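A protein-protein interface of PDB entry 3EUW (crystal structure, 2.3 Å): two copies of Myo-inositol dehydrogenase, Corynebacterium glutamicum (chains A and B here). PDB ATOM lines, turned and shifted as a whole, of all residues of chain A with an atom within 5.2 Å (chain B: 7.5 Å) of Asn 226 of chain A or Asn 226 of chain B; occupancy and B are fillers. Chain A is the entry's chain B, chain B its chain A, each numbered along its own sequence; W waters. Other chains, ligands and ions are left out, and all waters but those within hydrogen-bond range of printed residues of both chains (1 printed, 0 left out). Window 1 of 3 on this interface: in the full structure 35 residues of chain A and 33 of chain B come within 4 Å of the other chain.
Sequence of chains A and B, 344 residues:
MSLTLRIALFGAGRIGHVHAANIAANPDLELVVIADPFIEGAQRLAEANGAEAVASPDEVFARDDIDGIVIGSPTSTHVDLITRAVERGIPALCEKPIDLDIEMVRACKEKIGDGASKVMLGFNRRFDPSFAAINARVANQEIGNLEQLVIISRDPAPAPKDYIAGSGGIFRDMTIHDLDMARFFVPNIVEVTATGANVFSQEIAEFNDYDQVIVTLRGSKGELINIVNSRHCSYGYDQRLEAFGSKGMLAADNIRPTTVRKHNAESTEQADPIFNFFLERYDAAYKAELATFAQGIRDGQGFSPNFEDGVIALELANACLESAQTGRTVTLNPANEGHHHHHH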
ATOM      1  N   LEU A 149     -14.666 -18.418  -4.493  1.00  0.00           N
ATOM      2  CA  LEU A 149     -15.116 -17.040  -4.377  1.00  0.00           C
ATOM      3  C   LEU A 149     -14.300 -16.456  -3.236  1.00  0.00           C
ATOM      4  O   LEU A 149     -14.373 -16.937  -2.101  1.00  0.00           O
ATOM      5  CB  LEU A 149     -16.612 -16.980  -4.053  1.00  0.00           C
ATOM      6  CG  LEU A 149     -17.249 -15.589  -4.055  1.00  0.00           C
ATOM      7  CD1 LEU A 149     -17.185 -15.016  -5.459  1.00  0.00           C
ATOM      8  CD2 LEU A 149     -18.702 -15.673  -3.601  1.00  0.00           C
ATOM      9  N   VAL A 150     -13.508 -15.434  -3.542  1.00  0.00           N
ATOM     10  CA  VAL A 150     -12.666 -14.794  -2.541  1.00  0.00           C
ATOM     11  C   VAL A 150     -13.092 -13.357  -2.324  1.00  0.00           C
ATOM     12  O   VAL A 150     -13.067 -12.547  -3.246  1.00  0.00           O
ATOM     13  CB  VAL A 150     -11.169 -14.809  -2.948  1.00  0.00           C
ATOM     14  CG1 VAL A 150     -10.310 -14.219  -1.806  1.00  0.00           C
ATOM     15  CG2 VAL A 150     -10.729 -16.235  -3.247  1.00  0.00           C
ATOM     16  N   ILE A 151     -13.476 -13.054  -1.089  1.00  0.00           N
ATOM     17  CA  ILE A 151     -13.930 -11.719  -0.727  1.00  0.00           C
ATOM     18  C   ILE A 151     -13.027 -11.140   0.341  1.00  0.00           C
ATOM     19  O   ILE A 151     -12.732 -11.788   1.358  1.00  0.00           O
ATOM     20  CB  ILE A 151     -15.379 -11.774  -0.220  1.00  0.00           C
ATOM     21  CG1 ILE A 151     -16.259 -12.398  -1.299  1.00  0.00           C
ATOM     22  CG2 ILE A 151     -15.868 -10.372   0.160  1.00  0.00           C
ATOM     23  CD1 ILE A 151     -17.619 -12.839  -0.798  1.00  0.00           C
ATOM     24  N   ILE A 214     -11.126 -14.680   9.260  1.00  0.00           N
ATOM     25  CA  ILE A 214     -11.019 -15.361   7.976  1.00  0.00           C
ATOM     26  C   ILE A 214     -12.124 -16.413   8.022  1.00  0.00           C
ATOM     27  O   ILE A 214     -12.195 -17.219   8.956  1.00  0.00           O
ATOM     28  CB  ILE A 214      -9.693 -16.153   7.772  1.00  0.00           C
ATOM     29  CG1 ILE A 214      -8.453 -15.258   7.873  1.00  0.00           C
ATOM     30  CG2 ILE A 214      -9.768 -16.866   6.419  1.00  0.00           C
ATOM     31  CD1 ILE A 214      -8.041 -14.561   6.587  1.00  0.00           C
ATOM     32  N   VAL A 215     -12.970 -16.410   7.007  1.00  0.00           N
ATOM     33  CA  VAL A 215     -14.074 -17.346   6.936  1.00  0.00           C
ATOM     34  C   VAL A 215     -13.998 -18.166   5.652  1.00  0.00           C
ATOM     35  O   VAL A 215     -13.676 -17.634   4.588  1.00  0.00           O
ATOM     36  CB  VAL A 215     -15.416 -16.573   6.963  1.00  0.00           C
ATOM     37  CG1 VAL A 215     -16.574 -17.504   6.677  1.00  0.00           C
ATOM     38  CG2 VAL A 215     -15.595 -15.885   8.328  1.00  0.00           C
ATOM     39  N   THR A 216     -14.273 -19.461   5.760  1.00  0.00           N
ATOM     40  CA  THR A 216     -14.284 -20.334   4.593  1.00  0.00           C
ATOM     41  C   THR A 216     -15.580 -21.160   4.578  1.00  0.00           C
ATOM     42  O   THR A 216     -15.834 -21.943   5.485  1.00  0.00           O
ATOM     43  CB  THR A 216     -13.059 -21.273   4.576  1.00  0.00           C
ATOM     44  OG1 THR A 216     -11.854 -20.488   4.599  1.00  0.00           O
ATOM     45  CG2 THR A 216     -13.065 -22.128   3.319  1.00  0.00           C
ATOM     46  N   LEU A 217     -16.399 -20.968   3.545  1.00  0.00           N
ATOM     47  CA  LEU A 217     -17.659 -21.691   3.420  1.00  0.00           C
ATOM     48  C   LEU A 217     -17.585 -22.759   2.334  1.00  0.00           C
ATOM     49  O   LEU A 217     -16.940 -22.560   1.304  1.00  0.00           O
ATOM     50  CB  LEU A 217     -18.792 -20.742   3.039  1.00  0.00           C
ATOM     51  CG  LEU A 217     -19.013 -19.417   3.759  1.00  0.00           C
ATOM     52  CD1 LEU A 217     -20.132 -18.655   3.051  1.00  0.00           C
ATOM     53  CD2 LEU A 217     -19.367 -19.679   5.210  1.00  0.00           C
ATOM     54  N   LEU A 224     -15.812 -23.285  -2.789  1.00  0.00           N
ATOM     55  CA  LEU A 224     -15.183 -22.775  -1.570  1.00  0.00           C
ATOM     56  C   LEU A 224     -15.238 -21.249  -1.597  1.00  0.00           C
ATOM     57  O   LEU A 224     -14.679 -20.621  -2.486  1.00  0.00           O
ATOM     58  CB  LEU A 224     -13.730 -23.247  -1.445  1.00  0.00           C
ATOM     59  CG  LEU A 224     -13.549 -24.752  -1.222  1.00  0.00           C
ATOM     60  CD1 LEU A 224     -12.059 -25.092  -1.192  1.00  0.00           C
ATOM     61  CD2 LEU A 224     -14.232 -25.168   0.087  1.00  0.00           C
ATOM     62  N   ILE A 225     -15.942 -20.666  -0.634  1.00  0.00           N
ATOM     63  CA  ILE A 225     -16.045 -19.210  -0.525  1.00  0.00           C
ATOM     64  C   ILE A 225     -15.100 -18.798   0.612  1.00  0.00           C
ATOM     65  O   ILE A 225     -15.193 -19.310   1.723  1.00  0.00           O
ATOM     66  CB  ILE A 225     -17.493 -18.776  -0.198  1.00  0.00           C
ATOM     67  CG1 ILE A 225     -18.436 -19.271  -1.300  1.00  0.00           C
ATOM     68  CG2 ILE A 225     -17.599 -17.259  -0.101  1.00  0.00           C
ATOM     69  CD1 ILE A 225     -18.938 -20.681  -1.074  1.00  0.00           C
ATOM     70  N   ASN A 226     -14.183 -17.887   0.327  1.00  0.00           N
ATOM     71  CA  ASN A 226     -13.211 -17.451   1.317  1.00  0.00           C
ATOM     72  C   ASN A 226     -13.336 -15.952   1.588  1.00  0.00           C
ATOM     73  O   ASN A 226     -13.152 -15.130   0.691  1.00  0.00           O
ATOM     74  CB  ASN A 226     -11.806 -17.797   0.818  1.00  0.00           C
ATOM     75  CG  ASN A 226     -10.743 -17.472   1.820  1.00  0.00           C
ATOM     76  OD1 ASN A 226     -10.615 -18.133   2.847  1.00  0.00           O
ATOM     77  ND2 ASN A 226      -9.977 -16.435   1.538  1.00  0.00           N
ATOM     78  N   ILE A 227     -13.657 -15.609   2.831  1.00  0.00           N
ATOM     79  CA  ILE A 227     -13.829 -14.215   3.222  1.00  0.00           C
ATOM     80  C   ILE A 227     -12.743 -13.749   4.193  1.00  0.00           C
ATOM     81  O   ILE A 227     -12.492 -14.396   5.202  1.00  0.00           O
ATOM     82  CB  ILE A 227     -15.191 -14.005   3.903  1.00  0.00           C
ATOM     83  CG1 ILE A 227     -16.322 -14.376   2.933  1.00  0.00           C
ATOM     84  CG2 ILE A 227     -15.327 -12.563   4.367  1.00  0.00           C
ATOM     85  CD1 ILE A 227     -17.689 -14.481   3.596  1.00  0.00           C
ATOM     86  N   VAL A 228     -12.115 -12.624   3.872  1.00  0.00           N
ATOM     87  CA  VAL A 228     -11.089 -12.035   4.715  1.00  0.00           C
ATOM     88  C   VAL A 228     -11.595 -10.672   5.204  1.00  0.00           C
ATOM     89  O   VAL A 228     -12.015  -9.842   4.404  1.00  0.00           O
ATOM     90  CB  VAL A 228      -9.773 -11.850   3.933  1.00  0.00           C
ATOM     91  CG1 VAL A 228      -8.728 -11.120   4.795  1.00  0.00           C
ATOM     92  CG2 VAL A 228      -9.247 -13.216   3.512  1.00  0.00           C
ATOM     93  N   GLN B 148      -2.013  -9.821   8.227  1.00  0.00           N
ATOM     94  CA  GLN B 148      -2.596 -10.832   7.357  1.00  0.00           C
ATOM     95  C   GLN B 148      -1.667 -11.099   6.186  1.00  0.00           C
ATOM     96  O   GLN B 148      -0.981 -10.190   5.706  1.00  0.00           O
ATOM     97  CB  GLN B 148      -3.942 -10.359   6.813  1.00  0.00           C
ATOM     98  CG  GLN B 148      -4.868  -9.807   7.853  1.00  0.00           C
ATOM     99  CD  GLN B 148      -6.234  -9.472   7.291  1.00  0.00           C
ATOM    100  OE1 GLN B 148      -6.362  -8.973   6.168  1.00  0.00           O
ATOM    101  NE2 GLN B 148      -7.266  -9.729   8.080  1.00  0.00           N
ATOM    102  N   LEU B 149      -1.662 -12.346   5.724  1.00  0.00           N
ATOM    103  CA  LEU B 149      -0.839 -12.757   4.596  1.00  0.00           C
ATOM    104  C   LEU B 149      -1.758 -13.625   3.738  1.00  0.00           C
ATOM    105  O   LEU B 149      -2.195 -14.688   4.169  1.00  0.00           O
ATOM    106  CB  LEU B 149       0.372 -13.551   5.089  1.00  0.00           C
ATOM    107  CG  LEU B 149       1.446 -13.893   4.054  1.00  0.00           C
ATOM    108  CD1 LEU B 149       2.045 -12.619   3.462  1.00  0.00           C
ATOM    109  CD2 LEU B 149       2.529 -14.718   4.717  1.00  0.00           C
ATOM    110  N   VAL B 150      -2.067 -13.157   2.532  1.00  0.00           N
ATOM    111  CA  VAL B 150      -2.964 -13.883   1.650  1.00  0.00           C
ATOM    112  C   VAL B 150      -2.204 -14.402   0.451  1.00  0.00           C
ATOM    113  O   VAL B 150      -1.603 -13.639  -0.297  1.00  0.00           O
ATOM    114  CB  VAL B 150      -4.110 -12.985   1.184  1.00  0.00           C
ATOM    115  CG1 VAL B 150      -5.075 -13.783   0.324  1.00  0.00           C
ATOM    116  CG2 VAL B 150      -4.825 -12.395   2.398  1.00  0.00           C
ATOM    117  N   ILE B 151      -2.227 -15.717   0.287  1.00  0.00           N
ATOM    118  CA  ILE B 151      -1.506 -16.359  -0.797  1.00  0.00           C
ATOM    119  C   ILE B 151      -2.452 -17.116  -1.704  1.00  0.00           C
ATOM    120  O   ILE B 151      -3.306 -17.867  -1.241  1.00  0.00           O
ATOM    121  CB  ILE B 151      -0.442 -17.319  -0.224  1.00  0.00           C
ATOM    122  CG1 ILE B 151       0.467 -16.539   0.737  1.00  0.00           C
ATOM    123  CG2 ILE B 151       0.376 -17.941  -1.350  1.00  0.00           C
ATOM    124  CD1 ILE B 151       1.525 -17.377   1.465  1.00  0.00           C
ATOM    125  N   ILE B 152      -2.314 -16.893  -3.004  1.00  0.00           N
ATOM    126  CA  ILE B 152      -3.161 -17.569  -3.972  1.00  0.00           C
ATOM    127  C   ILE B 152      -2.294 -18.228  -5.016  1.00  0.00           C
ATOM    128  O   ILE B 152      -1.659 -17.560  -5.845  1.00  0.00           O
ATOM    129  CB  ILE B 152      -4.134 -16.593  -4.657  1.00  0.00           C
ATOM    130  CG1 ILE B 152      -5.053 -15.965  -3.603  1.00  0.00           C
ATOM    131  CG2 ILE B 152      -4.943 -17.331  -5.733  1.00  0.00           C
ATOM    132  CD1 ILE B 152      -6.037 -14.933  -4.142  1.00  0.00           C
ATOM    133  N   ASP B 178       3.553 -22.982  -0.209  1.00  0.00           N
ATOM    134  CA  ASP B 178       2.875 -21.838   0.388  1.00  0.00           C
ATOM    135  C   ASP B 178       3.039 -21.832   1.908  1.00  0.00           C
ATOM    136  O   ASP B 178       3.069 -20.781   2.537  1.00  0.00           O
ATOM    137  CB  ASP B 178       1.385 -21.874   0.045  1.00  0.00           C
ATOM    138  CG  ASP B 178       1.130 -21.872  -1.450  1.00  0.00           C
ATOM    139  OD1 ASP B 178       1.598 -20.948  -2.143  1.00  0.00           O
ATOM    140  OD2 ASP B 178       0.447 -22.792  -1.933  1.00  0.00           O
ATOM    141  N   ALA B 182       4.758 -18.907   4.038  1.00  0.00           N
ATOM    142  CA  ALA B 182       4.100 -18.377   5.204  1.00  0.00           C
ATOM    143  C   ALA B 182       5.104 -18.237   6.363  1.00  0.00           C
ATOM    144  O   ALA B 182       5.153 -17.194   7.002  1.00  0.00           O
ATOM    145  CB  ALA B 182       2.949 -19.275   5.598  1.00  0.00           C
ATOM    146  N   THR B 193      -5.705 -24.626  10.200  1.00  0.00           N
ATOM    147  CA  THR B 193      -7.067 -24.939   9.780  1.00  0.00           C
ATOM    148  C   THR B 193      -7.063 -25.127   8.266  1.00  0.00           C
ATOM    149  O   THR B 193      -6.498 -24.314   7.541  1.00  0.00           O
ATOM    150  CB  THR B 193      -8.034 -23.811  10.156  1.00  0.00           C
ATOM    151  OG1 THR B 193      -7.861 -23.492  11.539  1.00  0.00           O
ATOM    152  CG2 THR B 193      -9.472 -24.242   9.948  1.00  0.00           C
ATOM    153  N   ILE B 214      -8.337 -24.504   0.958  1.00  0.00           N
ATOM    154  CA  ILE B 214      -8.161 -23.190   1.572  1.00  0.00           C
ATOM    155  C   ILE B 214      -7.543 -23.482   2.927  1.00  0.00           C
ATOM    156  O   ILE B 214      -8.020 -24.350   3.655  1.00  0.00           O
ATOM    157  CB  ILE B 214      -9.481 -22.431   1.842  1.00  0.00           C
ATOM    158  CG1 ILE B 214      -9.960 -21.662   0.607  1.00  0.00           C
ATOM    159  CG2 ILE B 214      -9.234 -21.376   2.938  1.00  0.00           C
ATOM    160  CD1 ILE B 214     -10.153 -22.460  -0.609  1.00  0.00           C
ATOM    161  N   VAL B 215      -6.487 -22.765   3.269  1.00  0.00           N
ATOM    162  CA  VAL B 215      -5.828 -22.949   4.554  1.00  0.00           C
ATOM    163  C   VAL B 215      -5.747 -21.629   5.319  1.00  0.00           C
ATOM    164  O   VAL B 215      -5.525 -20.569   4.729  1.00  0.00           O
ATOM    165  CB  VAL B 215      -4.395 -23.491   4.367  1.00  0.00           C
ATOM    166  CG1 VAL B 215      -3.655 -23.488   5.698  1.00  0.00           C
ATOM    167  CG2 VAL B 215      -4.437 -24.910   3.781  1.00  0.00           C
ATOM    168  N   THR B 216      -5.954 -21.689   6.626  1.00  0.00           N
ATOM    169  CA  THR B 216      -5.834 -20.509   7.466  1.00  0.00           C
ATOM    170  C   THR B 216      -4.956 -20.862   8.677  1.00  0.00           C
ATOM    171  O   THR B 216      -5.308 -21.720   9.483  1.00  0.00           O
ATOM    172  CB  THR B 216      -7.215 -19.997   7.935  1.00  0.00           C
ATOM    173  OG1 THR B 216      -7.998 -19.629   6.796  1.00  0.00           O
ATOM    174  CG2 THR B 216      -7.060 -18.780   8.800  1.00  0.00           C
ATOM    175  N   LEU B 217      -3.803 -20.209   8.780  1.00  0.00           N
ATOM    176  CA  LEU B 217      -2.867 -20.460   9.881  1.00  0.00           C
ATOM    177  C   LEU B 217      -2.891 -19.306  10.880  1.00  0.00           C
ATOM    178  O   LEU B 217      -3.053 -18.148  10.491  1.00  0.00           O
ATOM    179  CB  LEU B 217      -1.435 -20.591   9.351  1.00  0.00           C
ATOM    180  CG  LEU B 217      -1.142 -21.500   8.157  1.00  0.00           C
ATOM    181  CD1 LEU B 217       0.275 -21.250   7.670  1.00  0.00           C
ATOM    182  CD2 LEU B 217      -1.330 -22.957   8.550  1.00  0.00           C
ATOM    183  N   GLU B 223      -1.353 -13.166  13.939  1.00  0.00           N
ATOM    184  CA  GLU B 223      -1.311 -13.001  12.494  1.00  0.00           C
ATOM    185  C   GLU B 223      -2.161 -14.103  11.869  1.00  0.00           C
ATOM    186  O   GLU B 223      -2.223 -15.224  12.389  1.00  0.00           O
ATOM    187  CB  GLU B 223       0.119 -13.121  11.958  1.00  0.00           C
ATOM    188  CG  GLU B 223       1.118 -12.194  12.609  1.00  0.00           C
ATOM    189  CD  GLU B 223       1.915 -12.876  13.707  1.00  0.00           C
ATOM    190  OE1 GLU B 223       1.353 -13.751  14.410  1.00  0.00           O
ATOM    191  OE2 GLU B 223       3.099 -12.528  13.875  1.00  0.00           O
ATOM    192  N   LEU B 224      -2.822 -13.784  10.763  1.00  0.00           N
ATOM    193  CA  LEU B 224      -3.640 -14.763  10.053  1.00  0.00           C
ATOM    194  C   LEU B 224      -3.068 -14.948   8.663  1.00  0.00           C
ATOM    195  O   LEU B 224      -2.982 -13.992   7.883  1.00  0.00           O
ATOM    196  CB  LEU B 224      -5.104 -14.303   9.953  1.00  0.00           C
ATOM    197  CG  LEU B 224      -5.848 -14.243  11.300  1.00  0.00           C
ATOM    198  CD1 LEU B 224      -7.277 -13.747  11.081  1.00  0.00           C
ATOM    199  CD2 LEU B 224      -5.851 -15.637  11.961  1.00  0.00           C
ATOM    200  N   ILE B 225      -2.647 -16.170   8.359  1.00  0.00           N
ATOM    201  CA  ILE B 225      -2.102 -16.470   7.048  1.00  0.00           C
ATOM    202  C   ILE B 225      -3.177 -17.283   6.325  1.00  0.00           C
ATOM    203  O   ILE B 225      -3.599 -18.338   6.803  1.00  0.00           O
ATOM    204  CB  ILE B 225      -0.809 -17.299   7.142  1.00  0.00           C
ATOM    205  CG1 ILE B 225       0.283 -16.516   7.888  1.00  0.00           C
ATOM    206  CG2 ILE B 225      -0.317 -17.618   5.750  1.00  0.00           C
ATOM    207  CD1 ILE B 225       0.145 -16.538   9.380  1.00  0.00           C
ATOM    208  N   ASN B 226      -3.620 -16.787   5.178  1.00  0.00           N
ATOM    209  CA  ASN B 226      -4.678 -17.447   4.416  1.00  0.00           C
ATOM    210  C   ASN B 226      -4.164 -17.889   3.042  1.00  0.00           C
ATOM    211  O   ASN B 226      -3.746 -17.075   2.217  1.00  0.00           O
ATOM    212  CB  ASN B 226      -5.860 -16.480   4.293  1.00  0.00           C
ATOM    213  CG  ASN B 226      -7.070 -17.106   3.640  1.00  0.00           C
ATOM    214  OD1 ASN B 226      -7.597 -18.114   4.103  1.00  0.00           O
ATOM    215  ND2 ASN B 226      -7.518 -16.501   2.557  1.00  0.00           N
ATOM    216  N   ILE B 227      -4.191 -19.196   2.810  1.00  0.00           N
ATOM    217  CA  ILE B 227      -3.705 -19.769   1.568  1.00  0.00           C
ATOM    218  C   ILE B 227      -4.809 -20.397   0.730  1.00  0.00           C
ATOM    219  O   ILE B 227      -5.599 -21.204   1.234  1.00  0.00           O
ATOM    220  CB  ILE B 227      -2.638 -20.854   1.856  1.00  0.00           C
ATOM    221  CG1 ILE B 227      -1.492 -20.247   2.673  1.00  0.00           C
ATOM    222  CG2 ILE B 227      -2.107 -21.435   0.553  1.00  0.00           C
ATOM    223  CD1 ILE B 227      -0.488 -21.278   3.184  1.00  0.00           C
ATOM    224  N   VAL B 228      -4.852 -20.014  -0.547  1.00  0.00           N
ATOM    225  CA  VAL B 228      -5.830 -20.529  -1.500  1.00  0.00           C
ATOM    226  C   VAL B 228      -5.122 -21.295  -2.631  1.00  0.00           C
ATOM    227  O   VAL B 228      -4.249 -20.755  -3.319  1.00  0.00           O
ATOM    228  CB  VAL B 228      -6.685 -19.385  -2.117  1.00  0.00           C
ATOM    229  CG1 VAL B 228      -7.689 -19.965  -3.120  1.00  0.00           C
ATOM    230  CG2 VAL B 228      -7.430 -18.611  -1.007  1.00  0.00           C
ATOM    231  N   ARG B 240       0.078 -15.293  -6.610  1.00  0.00           N
ATOM    232  CA  ARG B 240      -0.059 -13.989  -5.998  1.00  0.00           C
ATOM    233  C   ARG B 240       0.148 -14.051  -4.497  1.00  0.00           C
ATOM    234  O   ARG B 240      -0.085 -15.086  -3.858  1.00  0.00           O
ATOM    235  CB  ARG B 240      -1.436 -13.401  -6.318  1.00  0.00           C
ATOM    236  CG  ARG B 240      -1.588 -12.929  -7.760  1.00  0.00           C
ATOM    237  CD  ARG B 240      -3.020 -12.475  -8.032  1.00  0.00           C
ATOM    238  NE  ARG B 240      -3.929 -13.610  -8.151  1.00  0.00           N
ATOM    239  CZ  ARG B 240      -5.188 -13.622  -7.716  1.00  0.00           C
ATOM    240  NH1 ARG B 240      -5.693 -12.554  -7.107  1.00  0.00           N
ATOM    241  NH2 ARG B 240      -5.958 -14.689  -7.920  1.00  0.00           N
ATOM    242  N   GLU B 242      -0.153 -11.338  -0.927  1.00  0.00           N
ATOM    243  CA  GLU B 242      -0.519 -10.053  -0.372  1.00  0.00           C
ATOM    244  C   GLU B 242      -0.197 -10.026   1.122  1.00  0.00           C
ATOM    245  O   GLU B 242      -0.600 -10.921   1.863  1.00  0.00           O
ATOM    246  CB  GLU B 242      -2.019  -9.835  -0.594  1.00  0.00           C
ATOM    247  CG  GLU B 242      -2.586  -8.564  -0.011  1.00  0.00           C
ATOM    248  CD  GLU B 242      -4.111  -8.508  -0.104  1.00  0.00           C
ATOM    249  OE1 GLU B 242      -4.680  -8.932  -1.133  1.00  0.00           O
ATOM    250  OE2 GLU B 242      -4.745  -8.031   0.850  1.00  0.00           O
HETATM  251  O   HOH W   1     -10.228 -20.971   6.663  1.00  0.00           O
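Of the 20 printed residues of chain B, 5 touch a printed residue of chain A. Hydrophobic or aromatic side chains of chain B within 4 Å of the printed part of chain A: Ile 214 and Leu 224. Of the 12 printed residues of chain A, 5 touch a printed residue of chain B. Hydrophobic or aromatic side chains of chain A within 4 Å of the printed part of chain B: Ile 214, Leu 224 and Val 228. Among the printed residues, 9 pairs touch across the chains.
Among the printed residues, merely in contact across the chains: Ile 214 of chain A with Thr 216 of chain B (3.3 Å), Ile 214 of chain A with Leu 224 of chain B (3.7 Å), Ile 214 of chain A with Asn 226 of chain B (3.4 Å), Thr 216 of chain A with Ile 214 of chain B (3.2 Å), Leu 224 of chain A with Ile 214 of chain B (3.3 Å), Asn 226 of chain A with Ile 214 of chain B (3.5 Å), Val 228 of chain A with Gln 148 of chain B (3.5 Å) and Val 228 of chain A with Asn 226 of chain B (3.8 Å).
Water W1 lies within hydrogen-bond range of the side-chain hydroxyl of Thr 216 of chain B (2.6 Å) and the side-chain hydroxyl of Thr 216 of chain A (2.7 Å).
OG1 of Thr 216 of chain A is in hydrogen-bond range of OD1 of Asn 226 of chain A (3.2 Å). The side-chain hydroxyl (OG1) of Thr 216 of chain B is in hydrogen-bond range of the side-chain amide oxygen (OD1) of Asn 226 of chain B, at 3.1 Å. The backbone NH (N) of Asn 226 of chain A is in hydrogen-bond range of the backbone carbonyl oxygen (O) of Leu 149 of chain A, at 2.6 Å. The backbone NH (N) of Leu 149 of chain B lies within hydrogen-bond range of the backbone carbonyl oxygen (O) of Leu 224 of chain B, 3.0 Å away. The backbone NH (N) of Ile 151 of chain B lies within hydrogen-bond range of the backbone carbonyl oxygen (O) of Asn 226 of chain B, 2.8 Å away. O of Val 215 of chain B lies close to OD1 of Asn 226 of chain B (3.3 Å).
Ile 214 of chain A touches Thr 216 of chain B, and with the chains exchanged Thr 216 of chain A touches Ile 214 of chain B. Ile 214 of chain A touches Asn 226 of chain B, and with the chains exchanged Asn 226 of chain A touches Ile 214 of chain B. Asn 226 of chain B touches its own counterpart, Asn 226 of chain A. Val 228 of chain A touches Asn 226 of chain B, but with the chains exchanged Asn 226 of chain A does not touch Val 228 of chain B (4.2 Å). Of the 9 pairs that touch across the chains among the printed residues, 7 have their exchanged pair printed and touching as well.
ND2 of Asn 226 of chain B lies close to ND2 of Asn 226 of chain A, at 2.7 Å.
Asn 226 of chain A touches two residues of chain B. Printed residues of chain A within 4 Å of Asn 226 of chain B: Ile 214 (3.4 Å), Asn 226 (2.7 Å) and Val 228 (3.8 Å). Of the printed residues of chain A, Gln 148 of chain B touches Val 228 (3.5 Å). Printed residues of chain B within 4 Å of Leu 224 of chain A: Ile 214 (3.3 Å). Thr 193 of chain B touches none of the printed residues of chain A. Ile 151 of chain A touches none of the printed residues of chain B.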
